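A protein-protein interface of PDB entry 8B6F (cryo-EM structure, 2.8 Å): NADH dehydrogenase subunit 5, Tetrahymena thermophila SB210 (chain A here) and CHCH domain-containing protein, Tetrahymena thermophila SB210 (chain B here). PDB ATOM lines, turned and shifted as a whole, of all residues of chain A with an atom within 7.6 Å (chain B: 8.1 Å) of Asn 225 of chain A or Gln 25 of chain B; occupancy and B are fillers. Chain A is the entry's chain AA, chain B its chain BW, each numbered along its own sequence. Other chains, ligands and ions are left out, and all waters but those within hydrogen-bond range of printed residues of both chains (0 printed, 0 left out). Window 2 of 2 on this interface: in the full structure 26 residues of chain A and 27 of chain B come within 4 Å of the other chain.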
ATOM      1  N   ASN A 219     -19.686  -3.655  -6.798  1.00  0.00           N
ATOM      2  CA  ASN A 219     -20.593  -4.650  -7.359  1.00  0.00           C
ATOM      3  C   ASN A 219     -21.803  -3.996  -8.011  1.00  0.00           C
ATOM      4  O   ASN A 219     -22.226  -4.400  -9.100  1.00  0.00           O
ATOM      5  CB  ASN A 219     -21.038  -5.623  -6.267  1.00  0.00           C
ATOM      6  CG  ASN A 219     -22.097  -6.590  -6.749  1.00  0.00           C
ATOM      7  OD1 ASN A 219     -21.792  -7.599  -7.381  1.00  0.00           O
ATOM      8  ND2 ASN A 219     -23.355  -6.288  -6.448  1.00  0.00           N
ATOM      9  N   LEU A 220     -22.381  -2.985  -7.359  1.00  0.00           N
ATOM     10  CA  LEU A 220     -23.569  -2.339  -7.908  1.00  0.00           C
ATOM     11  C   LEU A 220     -23.247  -1.551  -9.170  1.00  0.00           C
ATOM     12  O   LEU A 220     -23.992  -1.612 -10.154  1.00  0.00           O
ATOM     13  CB  LEU A 220     -24.192  -1.423  -6.856  1.00  0.00           C
ATOM     14  CG  LEU A 220     -24.622  -2.082  -5.545  1.00  0.00           C
ATOM     15  CD1 LEU A 220     -25.223  -1.037  -4.635  1.00  0.00           C
ATOM     16  CD2 LEU A 220     -25.606  -3.216  -5.785  1.00  0.00           C
ATOM     17  N   ILE A 221     -22.146  -0.800  -9.165  1.00  0.00           N
ATOM     18  CA  ILE A 221     -21.850   0.065 -10.300  1.00  0.00           C
ATOM     19  C   ILE A 221     -21.490  -0.762 -11.528  1.00  0.00           C
ATOM     20  O   ILE A 221     -21.925  -0.459 -12.645  1.00  0.00           O
ATOM     21  CB  ILE A 221     -20.734   1.060  -9.931  1.00  0.00           C
ATOM     22  CG1 ILE A 221     -21.179   1.948  -8.768  1.00  0.00           C
ATOM     23  CG2 ILE A 221     -20.366   1.925 -11.128  1.00  0.00           C
ATOM     24  CD1 ILE A 221     -20.050   2.695  -8.104  1.00  0.00           C
ATOM     25  N   VAL A 222     -20.691  -1.813 -11.346  1.00  0.00           N
ATOM     26  CA  VAL A 222     -20.174  -2.553 -12.493  1.00  0.00           C
ATOM     27  C   VAL A 222     -21.282  -3.347 -13.174  1.00  0.00           C
ATOM     28  O   VAL A 222     -21.357  -3.394 -14.406  1.00  0.00           O
ATOM     29  CB  VAL A 222     -19.010  -3.459 -12.053  1.00  0.00           C
ATOM     30  CG1 VAL A 222     -18.577  -4.380 -13.188  1.00  0.00           C
ATOM     31  CG2 VAL A 222     -17.844  -2.618 -11.582  1.00  0.00           C
ATOM     32  N   SER A 223     -22.157  -3.982 -12.397  1.00  0.00           N
ATOM     33  CA  SER A 223     -23.137  -4.915 -12.942  1.00  0.00           C
ATOM     34  C   SER A 223     -24.578  -4.444 -12.815  1.00  0.00           C
ATOM     35  O   SER A 223     -25.377  -4.689 -13.720  1.00  0.00           O
ATOM     36  CB  SER A 223     -22.993  -6.281 -12.260  1.00  0.00           C
ATOM     37  OG  SER A 223     -23.143  -6.173 -10.856  1.00  0.00           O
ATOM     38  N   GLU A 224     -24.941  -3.774 -11.724  1.00  0.00           N
ATOM     39  CA  GLU A 224     -26.332  -3.420 -11.463  1.00  0.00           C
ATOM     40  C   GLU A 224     -26.760  -2.118 -12.124  1.00  0.00           C
ATOM     41  O   GLU A 224     -27.905  -1.696 -11.935  1.00  0.00           O
ATOM     42  CB  GLU A 224     -26.581  -3.323  -9.954  1.00  0.00           C
ATOM     43  CG  GLU A 224     -26.347  -4.602  -9.183  1.00  0.00           C
ATOM     44  CD  GLU A 224     -27.372  -5.661  -9.525  1.00  0.00           C
ATOM     45  OE1 GLU A 224     -28.338  -5.341 -10.246  1.00  0.00           O
ATOM     46  OE2 GLU A 224     -27.235  -6.803  -9.050  1.00  0.00           O
ATOM     47  N   ASN A 225     -25.877  -1.468 -12.880  1.00  0.00           N
ATOM     48  CA  ASN A 225     -26.208  -0.235 -13.596  1.00  0.00           C
ATOM     49  C   ASN A 225     -26.494   0.914 -12.630  1.00  0.00           C
ATOM     50  O   ASN A 225     -27.394   1.722 -12.858  1.00  0.00           O
ATOM     51  CB  ASN A 225     -27.390  -0.440 -14.548  1.00  0.00           C
ATOM     52  CG  ASN A 225     -27.098  -1.457 -15.631  1.00  0.00           C
ATOM     53  OD1 ASN A 225     -26.520  -1.129 -16.666  1.00  0.00           O
ATOM     54  ND2 ASN A 225     -27.502  -2.700 -15.400  1.00  0.00           N
ATOM     55  N   TYR A 226     -25.722   0.995 -11.552  1.00  0.00           N
ATOM     56  CA  TYR A 226     -25.812   2.091 -10.596  1.00  0.00           C
ATOM     57  C   TYR A 226     -24.683   3.080 -10.854  1.00  0.00           C
ATOM     58  O   TYR A 226     -23.510   2.696 -10.871  1.00  0.00           O
ATOM     59  CB  TYR A 226     -25.726   1.577  -9.158  1.00  0.00           C
ATOM     60  CG  TYR A 226     -27.020   1.055  -8.583  1.00  0.00           C
ATOM     61  CD1 TYR A 226     -27.881   1.895  -7.891  1.00  0.00           C
ATOM     62  CD2 TYR A 226     -27.368  -0.282  -8.703  1.00  0.00           C
ATOM     63  CE1 TYR A 226     -29.058   1.422  -7.350  1.00  0.00           C
ATOM     64  CE2 TYR A 226     -28.543  -0.767  -8.165  1.00  0.00           C
ATOM     65  CZ  TYR A 226     -29.385   0.091  -7.490  1.00  0.00           C
ATOM     66  OH  TYR A 226     -30.556  -0.384  -6.951  1.00  0.00           O
ATOM     67  N   TYR A 227     -25.032   4.346 -11.058  1.00  0.00           N
ATOM     68  CA  TYR A 227     -24.034   5.402 -11.084  1.00  0.00           C
ATOM     69  C   TYR A 227     -24.651   6.655 -10.488  1.00  0.00           C
ATOM     70  O   TYR A 227     -25.867   6.853 -10.550  1.00  0.00           O
ATOM     71  CB  TYR A 227     -23.502   5.669 -12.498  1.00  0.00           C
ATOM     72  CG  TYR A 227     -24.531   6.117 -13.505  1.00  0.00           C
ATOM     73  CD1 TYR A 227     -24.886   7.454 -13.619  1.00  0.00           C
ATOM     74  CD2 TYR A 227     -25.123   5.205 -14.368  1.00  0.00           C
ATOM     75  CE1 TYR A 227     -25.818   7.869 -14.550  1.00  0.00           C
ATOM     76  CE2 TYR A 227     -26.055   5.608 -15.301  1.00  0.00           C
ATOM     77  CZ  TYR A 227     -26.399   6.941 -15.388  1.00  0.00           C
ATOM     78  OH  TYR A 227     -27.327   7.344 -16.318  1.00  0.00           O
ATOM     79  N   TYR A 228     -23.804   7.493  -9.903  1.00  0.00           N
ATOM     80  CA  TYR A 228     -24.246   8.670  -9.176  1.00  0.00           C
ATOM     81  C   TYR A 228     -23.572   9.912  -9.735  1.00  0.00           C
ATOM     82  O   TYR A 228     -22.436   9.863 -10.212  1.00  0.00           O
ATOM     83  CB  TYR A 228     -23.935   8.547  -7.681  1.00  0.00           C
ATOM     84  CG  TYR A 228     -24.421   7.260  -7.064  1.00  0.00           C
ATOM     85  CD1 TYR A 228     -25.720   7.142  -6.592  1.00  0.00           C
ATOM     86  CD2 TYR A 228     -23.580   6.165  -6.949  1.00  0.00           C
ATOM     87  CE1 TYR A 228     -26.167   5.967  -6.027  1.00  0.00           C
ATOM     88  CE2 TYR A 228     -24.016   4.986  -6.385  1.00  0.00           C
ATOM     89  CZ  TYR A 228     -25.311   4.893  -5.925  1.00  0.00           C
ATOM     90  OH  TYR A 228     -25.752   3.720  -5.363  1.00  0.00           O
ATOM     91  N   ASP A 251     -19.406   6.666 -12.066  1.00  0.00           N
ATOM     92  CA  ASP A 251     -19.943   5.815 -13.115  1.00  0.00           C
ATOM     93  C   ASP A 251     -19.087   4.555 -13.215  1.00  0.00           C
ATOM     94  O   ASP A 251     -18.176   4.335 -12.412  1.00  0.00           O
ATOM     95  CB  ASP A 251     -19.985   6.579 -14.441  1.00  0.00           C
ATOM     96  CG  ASP A 251     -20.955   5.975 -15.437  1.00  0.00           C
ATOM     97  OD1 ASP A 251     -21.218   4.759 -15.349  1.00  0.00           O
ATOM     98  OD2 ASP A 251     -21.454   6.717 -16.309  1.00  0.00           O
ATOM     99  N   LEU A 252     -19.389   3.713 -14.205  1.00  0.00           N
ATOM    100  CA  LEU A 252     -18.551   2.541 -14.431  1.00  0.00           C
ATOM    101  C   LEU A 252     -17.139   2.951 -14.826  1.00  0.00           C
ATOM    102  O   LEU A 252     -16.159   2.367 -14.352  1.00  0.00           O
ATOM    103  CB  LEU A 252     -19.168   1.637 -15.499  1.00  0.00           C
ATOM    104  CG  LEU A 252     -18.353   0.387 -15.852  1.00  0.00           C
ATOM    105  CD1 LEU A 252     -19.268  -0.752 -16.241  1.00  0.00           C
ATOM    106  CD2 LEU A 252     -17.357   0.643 -16.975  1.00  0.00           C
ATOM    107  N   SER A 673     -23.235  -9.278 -18.726  1.00  0.00           N
ATOM    108  CA  SER A 673     -23.852  -8.647 -17.566  1.00  0.00           C
ATOM    109  C   SER A 673     -23.119  -7.385 -17.127  1.00  0.00           C
ATOM    110  O   SER A 673     -23.298  -6.936 -15.992  1.00  0.00           O
ATOM    111  CB  SER A 673     -23.929  -9.638 -16.404  1.00  0.00           C
ATOM    112  OG  SER A 673     -22.635 -10.059 -16.012  1.00  0.00           O
ATOM    113  N   LEU A 674     -22.294  -6.804 -17.992  1.00  0.00           N
ATOM    114  CA  LEU A 674     -21.623  -5.559 -17.658  1.00  0.00           C
ATOM    115  C   LEU A 674     -22.601  -4.395 -17.751  1.00  0.00           C
ATOM    116  O   LEU A 674     -23.584  -4.438 -18.496  1.00  0.00           O
ATOM    117  CB  LEU A 674     -20.434  -5.317 -18.587  1.00  0.00           C
ATOM    118  CG  LEU A 674     -19.453  -4.222 -18.161  1.00  0.00           C
ATOM    119  CD1 LEU A 674     -18.678  -4.635 -16.921  1.00  0.00           C
ATOM    120  CD2 LEU A 674     -18.504  -3.873 -19.294  1.00  0.00           C
ATOM    121  N   SER A 675     -22.328  -3.349 -16.978  1.00  0.00           N
ATOM    122  CA  SER A 675     -23.178  -2.171 -17.006  1.00  0.00           C
ATOM    123  C   SER A 675     -22.960  -1.394 -18.302  1.00  0.00           C
ATOM    124  O   SER A 675     -22.006  -1.619 -19.049  1.00  0.00           O
ATOM    125  CB  SER A 675     -22.900  -1.275 -15.801  1.00  0.00           C
ATOM    126  OG  SER A 675     -23.274  -1.915 -14.596  1.00  0.00           O
ATOM    127  N   ASP A 676     -23.873  -0.464 -18.562  1.00  0.00           N
ATOM    128  CA  ASP A 676     -23.821   0.311 -19.791  1.00  0.00           C
ATOM    129  C   ASP A 676     -22.562   1.168 -19.834  1.00  0.00           C
ATOM    130  O   ASP A 676     -22.181   1.792 -18.841  1.00  0.00           O
ATOM    131  CB  ASP A 676     -25.062   1.196 -19.889  1.00  0.00           C
ATOM    132  CG  ASP A 676     -25.190   1.881 -21.229  1.00  0.00           C
ATOM    133  OD1 ASP A 676     -24.403   1.566 -22.146  1.00  0.00           O
ATOM    134  OD2 ASP A 676     -26.079   2.747 -21.357  1.00  0.00           O
ATOM    135  N   LEU A 677     -21.911   1.189 -20.996  1.00  0.00           N
ATOM    136  CA  LEU A 677     -20.722   2.004 -21.205  1.00  0.00           C
ATOM    137  C   LEU A 677     -21.027   3.364 -21.816  1.00  0.00           C
ATOM    138  O   LEU A 677     -20.112   4.183 -21.953  1.00  0.00           O
ATOM    139  CB  LEU A 677     -19.737   1.256 -22.108  1.00  0.00           C
ATOM    140  CG  LEU A 677     -19.113  -0.004 -21.505  1.00  0.00           C
ATOM    141  CD1 LEU A 677     -18.443  -0.822 -22.585  1.00  0.00           C
ATOM    142  CD2 LEU A 677     -18.121   0.365 -20.424  1.00  0.00           C
ATOM    143  N   LYS A 678     -22.281   3.623 -22.183  1.00  0.00           N
ATOM    144  CA  LYS A 678     -22.694   4.914 -22.727  1.00  0.00           C
ATOM    145  C   LYS A 678     -21.991   5.231 -24.044  1.00  0.00           C
ATOM    146  O   LYS A 678     -21.695   6.390 -24.337  1.00  0.00           O
ATOM    147  CB  LYS A 678     -22.453   6.037 -21.714  1.00  0.00           C
ATOM    148  CG  LYS A 678     -22.991   5.741 -20.318  1.00  0.00           C
ATOM    149  CD  LYS A 678     -24.490   5.473 -20.336  1.00  0.00           C
ATOM    150  CE  LYS A 678     -25.014   5.180 -18.939  1.00  0.00           C
ATOM    151  NZ  LYS A 678     -26.482   4.927 -18.934  1.00  0.00           N
ATOM    152  N   LYS B  18     -39.639   0.068 -26.392  1.00  0.00           N
ATOM    153  CA  LYS B  18     -38.525   0.898 -25.947  1.00  0.00           C
ATOM    154  C   LYS B  18     -38.615   1.195 -24.456  1.00  0.00           C
ATOM    155  O   LYS B  18     -37.600   1.178 -23.751  1.00  0.00           O
ATOM    156  CB  LYS B  18     -38.486   2.195 -26.754  1.00  0.00           C
ATOM    157  CG  LYS B  18     -38.206   1.983 -28.236  1.00  0.00           C
ATOM    158  CD  LYS B  18     -38.336   3.275 -29.030  1.00  0.00           C
ATOM    159  CE  LYS B  18     -37.261   4.288 -28.668  1.00  0.00           C
ATOM    160  NZ  LYS B  18     -35.891   3.776 -28.948  1.00  0.00           N
ATOM    161  N   GLU B  19     -39.820   1.465 -23.954  1.00  0.00           N
ATOM    162  CA  GLU B  19     -39.977   1.708 -22.524  1.00  0.00           C
ATOM    163  C   GLU B  19     -39.591   0.475 -21.716  1.00  0.00           C
ATOM    164  O   GLU B  19     -38.947   0.588 -20.667  1.00  0.00           O
ATOM    165  CB  GLU B  19     -41.414   2.124 -22.209  1.00  0.00           C
ATOM    166  CG  GLU B  19     -41.787   3.518 -22.692  1.00  0.00           C
ATOM    167  CD  GLU B  19     -41.979   3.590 -24.191  1.00  0.00           C
ATOM    168  OE1 GLU B  19     -41.993   2.526 -24.843  1.00  0.00           O
ATOM    169  OE2 GLU B  19     -42.115   4.712 -24.720  1.00  0.00           O
ATOM    170  N   GLU B  20     -39.982  -0.710 -22.184  1.00  0.00           N
ATOM    171  CA  GLU B  20     -39.617  -1.937 -21.484  1.00  0.00           C
ATOM    172  C   GLU B  20     -38.112  -2.165 -21.515  1.00  0.00           C
ATOM    173  O   GLU B  20     -37.530  -2.624 -20.526  1.00  0.00           O
ATOM    174  CB  GLU B  20     -40.355  -3.128 -22.093  1.00  0.00           C
ATOM    175  CG  GLU B  20     -41.837  -3.154 -21.767  1.00  0.00           C
ATOM    176  CD  GLU B  20     -42.546  -4.338 -22.387  1.00  0.00           C
ATOM    177  OE1 GLU B  20     -41.921  -5.047 -23.200  1.00  0.00           O
ATOM    178  OE2 GLU B  20     -43.729  -4.562 -22.063  1.00  0.00           O
ATOM    179  N   ILE B  21     -37.462  -1.858 -22.639  1.00  0.00           N
ATOM    180  CA  ILE B  21     -36.010  -1.989 -22.710  1.00  0.00           C
ATOM    181  C   ILE B  21     -35.352  -1.042 -21.715  1.00  0.00           C
ATOM    182  O   ILE B  21     -34.432  -1.422 -20.985  1.00  0.00           O
ATOM    183  CB  ILE B  21     -35.515  -1.734 -24.145  1.00  0.00           C
ATOM    184  CG1 ILE B  21     -36.040  -2.819 -25.085  1.00  0.00           C
ATOM    185  CG2 ILE B  21     -33.989  -1.691 -24.190  1.00  0.00           C
ATOM    186  CD1 ILE B  21     -35.857  -2.502 -26.553  1.00  0.00           C
ATOM    187  N   GLU B  22     -35.822   0.205 -21.670  1.00  0.00           N
ATOM    188  CA  GLU B  22     -35.273   1.170 -20.723  1.00  0.00           C
ATOM    189  C   GLU B  22     -35.474   0.704 -19.288  1.00  0.00           C
ATOM    190  O   GLU B  22     -34.573   0.835 -18.451  1.00  0.00           O
ATOM    191  CB  GLU B  22     -35.917   2.539 -20.938  1.00  0.00           C
ATOM    192  CG  GLU B  22     -35.603   3.154 -22.292  1.00  0.00           C
ATOM    193  CD  GLU B  22     -36.484   4.347 -22.606  1.00  0.00           C
ATOM    194  OE1 GLU B  22     -37.318   4.714 -21.751  1.00  0.00           O
ATOM    195  OE2 GLU B  22     -36.344   4.917 -23.708  1.00  0.00           O
ATOM    196  N   ALA B  23     -36.653   0.159 -18.981  1.00  0.00           N
ATOM    197  CA  ALA B  23     -36.892  -0.390 -17.652  1.00  0.00           C
ATOM    198  C   ALA B  23     -35.897  -1.500 -17.343  1.00  0.00           C
ATOM    199  O   ALA B  23     -35.070  -1.378 -16.435  1.00  0.00           O
ATOM    200  CB  ALA B  23     -38.328  -0.903 -17.550  1.00  0.00           C
ATOM    201  N   TYR B  24     -35.950  -2.591 -18.106  1.00  0.00           N
ATOM    202  CA  TYR B  24     -34.967  -3.667 -17.988  1.00  0.00           C
ATOM    203  C   TYR B  24     -33.709  -3.280 -18.769  1.00  0.00           C
ATOM    204  O   TYR B  24     -33.242  -4.002 -19.648  1.00  0.00           O
ATOM    205  CB  TYR B  24     -35.536  -4.980 -18.508  1.00  0.00           C
ATOM    206  CG  TYR B  24     -36.986  -5.234 -18.173  1.00  0.00           C
ATOM    207  CD1 TYR B  24     -37.393  -5.460 -16.866  1.00  0.00           C
ATOM    208  CD2 TYR B  24     -37.946  -5.276 -19.174  1.00  0.00           C
ATOM    209  CE1 TYR B  24     -38.718  -5.703 -16.563  1.00  0.00           C
ATOM    210  CE2 TYR B  24     -39.272  -5.518 -18.884  1.00  0.00           C
ATOM    211  CZ  TYR B  24     -39.652  -5.732 -17.577  1.00  0.00           C
ATOM    212  OH  TYR B  24     -40.974  -5.975 -17.285  1.00  0.00           O
ATOM    213  N   GLN B  25     -33.168  -2.110 -18.427  1.00  0.00           N
ATOM    214  CA  GLN B  25     -32.096  -1.485 -19.194  1.00  0.00           C
ATOM    215  C   GLN B  25     -31.098  -2.511 -19.704  1.00  0.00           C
ATOM    216  O   GLN B  25     -30.529  -3.289 -18.933  1.00  0.00           O
ATOM    217  CB  GLN B  25     -31.384  -0.429 -18.337  1.00  0.00           C
ATOM    218  CG  GLN B  25     -30.608  -0.949 -17.131  1.00  0.00           C
ATOM    219  CD  GLN B  25     -31.493  -1.576 -16.078  1.00  0.00           C
ATOM    220  OE1 GLN B  25     -32.250  -2.502 -16.361  1.00  0.00           O
ATOM    221  NE2 GLN B  25     -31.412  -1.066 -14.854  1.00  0.00           N
ATOM    222  N   VAL B  26     -30.902  -2.512 -21.014  1.00  0.00           N
ATOM    223  CA  VAL B  26     -30.038  -3.465 -21.704  1.00  0.00           C
ATOM    224  C   VAL B  26     -28.776  -2.727 -22.127  1.00  0.00           C
ATOM    225  O   VAL B  26     -28.873  -1.609 -22.644  1.00  0.00           O
ATOM    226  CB  VAL B  26     -30.739  -4.083 -22.929  1.00  0.00           C
ATOM    227  CG1 VAL B  26     -29.829  -5.076 -23.634  1.00  0.00           C
ATOM    228  CG2 VAL B  26     -32.040  -4.750 -22.516  1.00  0.00           C
ATOM    229  N   PRO B  27     -27.587  -3.296 -21.926  1.00  0.00           N
ATOM    230  CA  PRO B  27     -26.374  -2.613 -22.383  1.00  0.00           C
ATOM    231  C   PRO B  27     -26.400  -2.410 -23.890  1.00  0.00           C
ATOM    232  O   PRO B  27     -26.951  -3.220 -24.638  1.00  0.00           O
ATOM    233  CB  PRO B  27     -25.245  -3.561 -21.958  1.00  0.00           C
ATOM    234  CG  PRO B  27     -25.897  -4.883 -21.790  1.00  0.00           C
ATOM    235  CD  PRO B  27     -27.280  -4.595 -21.304  1.00  0.00           C
ATOM    236  N   MET B  28     -25.801  -1.303 -24.331  1.00  0.00           N
ATOM    237  CA  MET B  28     -25.800  -0.992 -25.755  1.00  0.00           C
ATOM    238  C   MET B  28     -25.182  -2.119 -26.568  1.00  0.00           C
ATOM    239  O   MET B  28     -25.573  -2.339 -27.719  1.00  0.00           O
ATOM    240  CB  MET B  28     -25.048   0.314 -26.008  1.00  0.00           C
ATOM    241  CG  MET B  28     -25.193   0.847 -27.425  1.00  0.00           C
ATOM    242  SD  MET B  28     -26.890   1.282 -27.841  1.00  0.00           S
ATOM    243  CE  MET B  28     -26.700   1.773 -29.551  1.00  0.00           C
ATOM    244  N   LYS B  31     -28.076  -4.308 -27.091  1.00  0.00           N
ATOM    245  CA  LYS B  31     -29.159  -3.608 -27.770  1.00  0.00           C
ATOM    246  C   LYS B  31     -28.853  -3.396 -29.247  1.00  0.00           C
ATOM    247  O   LYS B  31     -29.774  -3.319 -30.067  1.00  0.00           O
ATOM    248  CB  LYS B  31     -29.428  -2.269 -27.081  1.00  0.00           C
ATOM    249  CG  LYS B  31     -30.650  -1.527 -27.604  1.00  0.00           C
ATOM    250  CD  LYS B  31     -30.279  -0.512 -28.675  1.00  0.00           C
ATOM    251  CE  LYS B  31     -31.502   0.251 -29.157  1.00  0.00           C
ATOM    252  NZ  LYS B  31     -31.155   1.245 -30.212  1.00  0.00           N
ATOM    253  N   VAL B  36     -32.305  -8.828 -28.438  1.00  0.00           N
ATOM    254  CA  VAL B  36     -32.869  -8.159 -27.271  1.00  0.00           C
ATOM    255  C   VAL B  36     -34.054  -8.947 -26.730  1.00  0.00           C
ATOM    256  O   VAL B  36     -34.221  -9.086 -25.513  1.00  0.00           O
ATOM    257  CB  VAL B  36     -33.260  -6.712 -27.620  1.00  0.00           C
ATOM    258  CG1 VAL B  36     -33.861  -6.010 -26.412  1.00  0.00           C
ATOM    259  CG2 VAL B  36     -32.053  -5.947 -28.133  1.00  0.00           C
ATOM    260  N   TYR B  39     -32.701 -11.802 -24.897  1.00  0.00           N
ATOM    261  CA  TYR B  39     -31.857 -11.393 -23.782  1.00  0.00           C
ATOM    262  C   TYR B  39     -32.679 -10.949 -22.579  1.00  0.00           C
ATOM    263  O   TYR B  39     -32.353 -11.300 -21.439  1.00  0.00           O
ATOM    264  CB  TYR B  39     -30.923 -10.267 -24.229  1.00  0.00           C
ATOM    265  CG  TYR B  39     -30.047  -9.707 -23.130  1.00  0.00           C
ATOM    266  CD1 TYR B  39     -28.847 -10.318 -22.792  1.00  0.00           C
ATOM    267  CD2 TYR B  39     -30.413  -8.557 -22.443  1.00  0.00           C
ATOM    268  CE1 TYR B  39     -28.041  -9.807 -21.794  1.00  0.00           C
ATOM    269  CE2 TYR B  39     -29.614  -8.038 -21.443  1.00  0.00           C
ATOM    270  CZ  TYR B  39     -28.428  -8.667 -21.126  1.00  0.00           C
ATOM    271  OH  TYR B  39     -27.628  -8.156 -20.131  1.00  0.00           O
ATOM    272  N   ILE B  40     -33.747 -10.183 -22.809  1.00  0.00           N
ATOM    273  CA  ILE B  40     -34.496  -9.605 -21.692  1.00  0.00           C
ATOM    274  C   ILE B  40     -35.043 -10.679 -20.759  1.00  0.00           C
ATOM    275  O   ILE B  40     -34.899 -10.532 -19.535  1.00  0.00           O
ATOM    276  CB  ILE B  40     -35.593  -8.666 -22.225  1.00  0.00           C
ATOM    277  CG1 ILE B  40     -34.956  -7.393 -22.788  1.00  0.00           C
ATOM    278  CG2 ILE B  40     -36.597  -8.325 -21.125  1.00  0.00           C
ATOM    279  CD1 ILE B  40     -35.922  -6.482 -23.510  1.00  0.00           C
ATOM    280  N   LYS B  43     -32.210 -11.825 -18.523  1.00  0.00           N
ATOM    281  CA  LYS B  43     -31.857 -10.838 -17.508  1.00  0.00           C
ATOM    282  C   LYS B  43     -32.902 -10.792 -16.401  1.00  0.00           C
ATOM    283  O   LYS B  43     -32.559 -10.688 -15.217  1.00  0.00           O
ATOM    284  CB  LYS B  43     -31.695  -9.459 -18.149  1.00  0.00           C
ATOM    285  CG  LYS B  43     -31.202  -8.389 -17.182  1.00  0.00           C
ATOM    286  CD  LYS B  43     -31.101  -7.035 -17.861  1.00  0.00           C
ATOM    287  CE  LYS B  43     -30.579  -5.976 -16.906  1.00  0.00           C
ATOM    288  NZ  LYS B  43     -29.187  -6.257 -16.464  1.00  0.00           N
ATOM    289  N   GLN B  47     -32.252 -11.541 -12.471  1.00  0.00           N
ATOM    290  CA  GLN B  47     -32.651 -10.602 -11.428  1.00  0.00           C
ATOM    291  C   GLN B  47     -33.537 -11.279 -10.393  1.00  0.00           C
ATOM    292  O   GLN B  47     -33.382 -11.055  -9.187  1.00  0.00           O
ATOM    293  CB  GLN B  47     -33.371  -9.409 -12.054  1.00  0.00           C
ATOM    294  CG  GLN B  47     -32.455  -8.464 -12.813  1.00  0.00           C
ATOM    295  CD  GLN B  47     -31.704  -7.518 -11.900  1.00  0.00           C
ATOM    296  OE1 GLN B  47     -32.101  -7.294 -10.758  1.00  0.00           O
ATOM    297  NE2 GLN B  47     -30.612  -6.955 -12.402  1.00  0.00           N
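Among the printed residues, pairs that only touch across the chains: Glu 224 of chain A with Gln 47 of chain B, Asn 225 of chain A with Gln 25 of chain B, Leu 674 of chain A with Pro 27 of chain B and Asp 676 of chain A with Met 28 of chain B.
Of chain B, only Gln 25 (3.9 Å) comes within 4 Å of Asn 225 of chain A. Gln 25 of chain B touches just one residue of chain A: Asn 225. Printed residues of chain B within 4 Å of Asp 676 of chain A: Met 28 (3.9 Å). Of the printed residues of chain A, Met 28 of chain B touches Asp 676. Of the printed residues of chain A, Pro 27 of chain B touches Leu 674. Of the printed residues of chain B, Glu 224 of chain A touches Gln 47. Of the printed residues of chain B, Leu 674 of chain A touches Pro 27 (3.9 Å). The nearest residue of chain B that does not touch Asn 225 of chain A is Lys 43 of chain B (4.1 Å). The nearest printed residue of chain A that does not touch Gln 47 of chain B is Ser 223 of chain A (5.9 Å).
Of the 17 printed residues of chain B, 4 touch a printed residue of chain A. Hydrophobic or aromatic side chains of chain B within 4 Å of the printed part of chain A: Pro 27. Of the 18 printed residues of chain A, 4 touch a printed residue of chain B. Printed residues of chain A that touch a printed residue of chain B: Glu 224, Asn 225, Leu 674 and Asp 676.
The backbone NH of Asn 225 of chain A lies within hydrogen-bond range of the side-chain hydroxyl of Ser 675 of chain A (3.1 Å). The side-chain carboxylate (OD2) of Asp 676 of chain A lies within salt-bridge range of the side-chain amino group (NZ) of Lys 678 of chain A, at 3.3 Å. N of Asp 676 of chain A sits at hydrogen-bond distance from OD1 of Asn 225 of chain A, at 3.3 Å. O of Ser 223 of chain A lies within hydrogen-bond range of ND2 of Asn 225 of chain A (3.4 Å). The backbone carbonyl oxygen (O) of Leu 220 of chain A lies within hydrogen-bond range of the backbone NH (N) of Asn 225 of chain A (3.3 Å). The backbone carbonyl oxygen of Ala 23 of chain B sits close to the side-chain amide oxygen of Gln 25 of chain B, at 3.0 Å.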
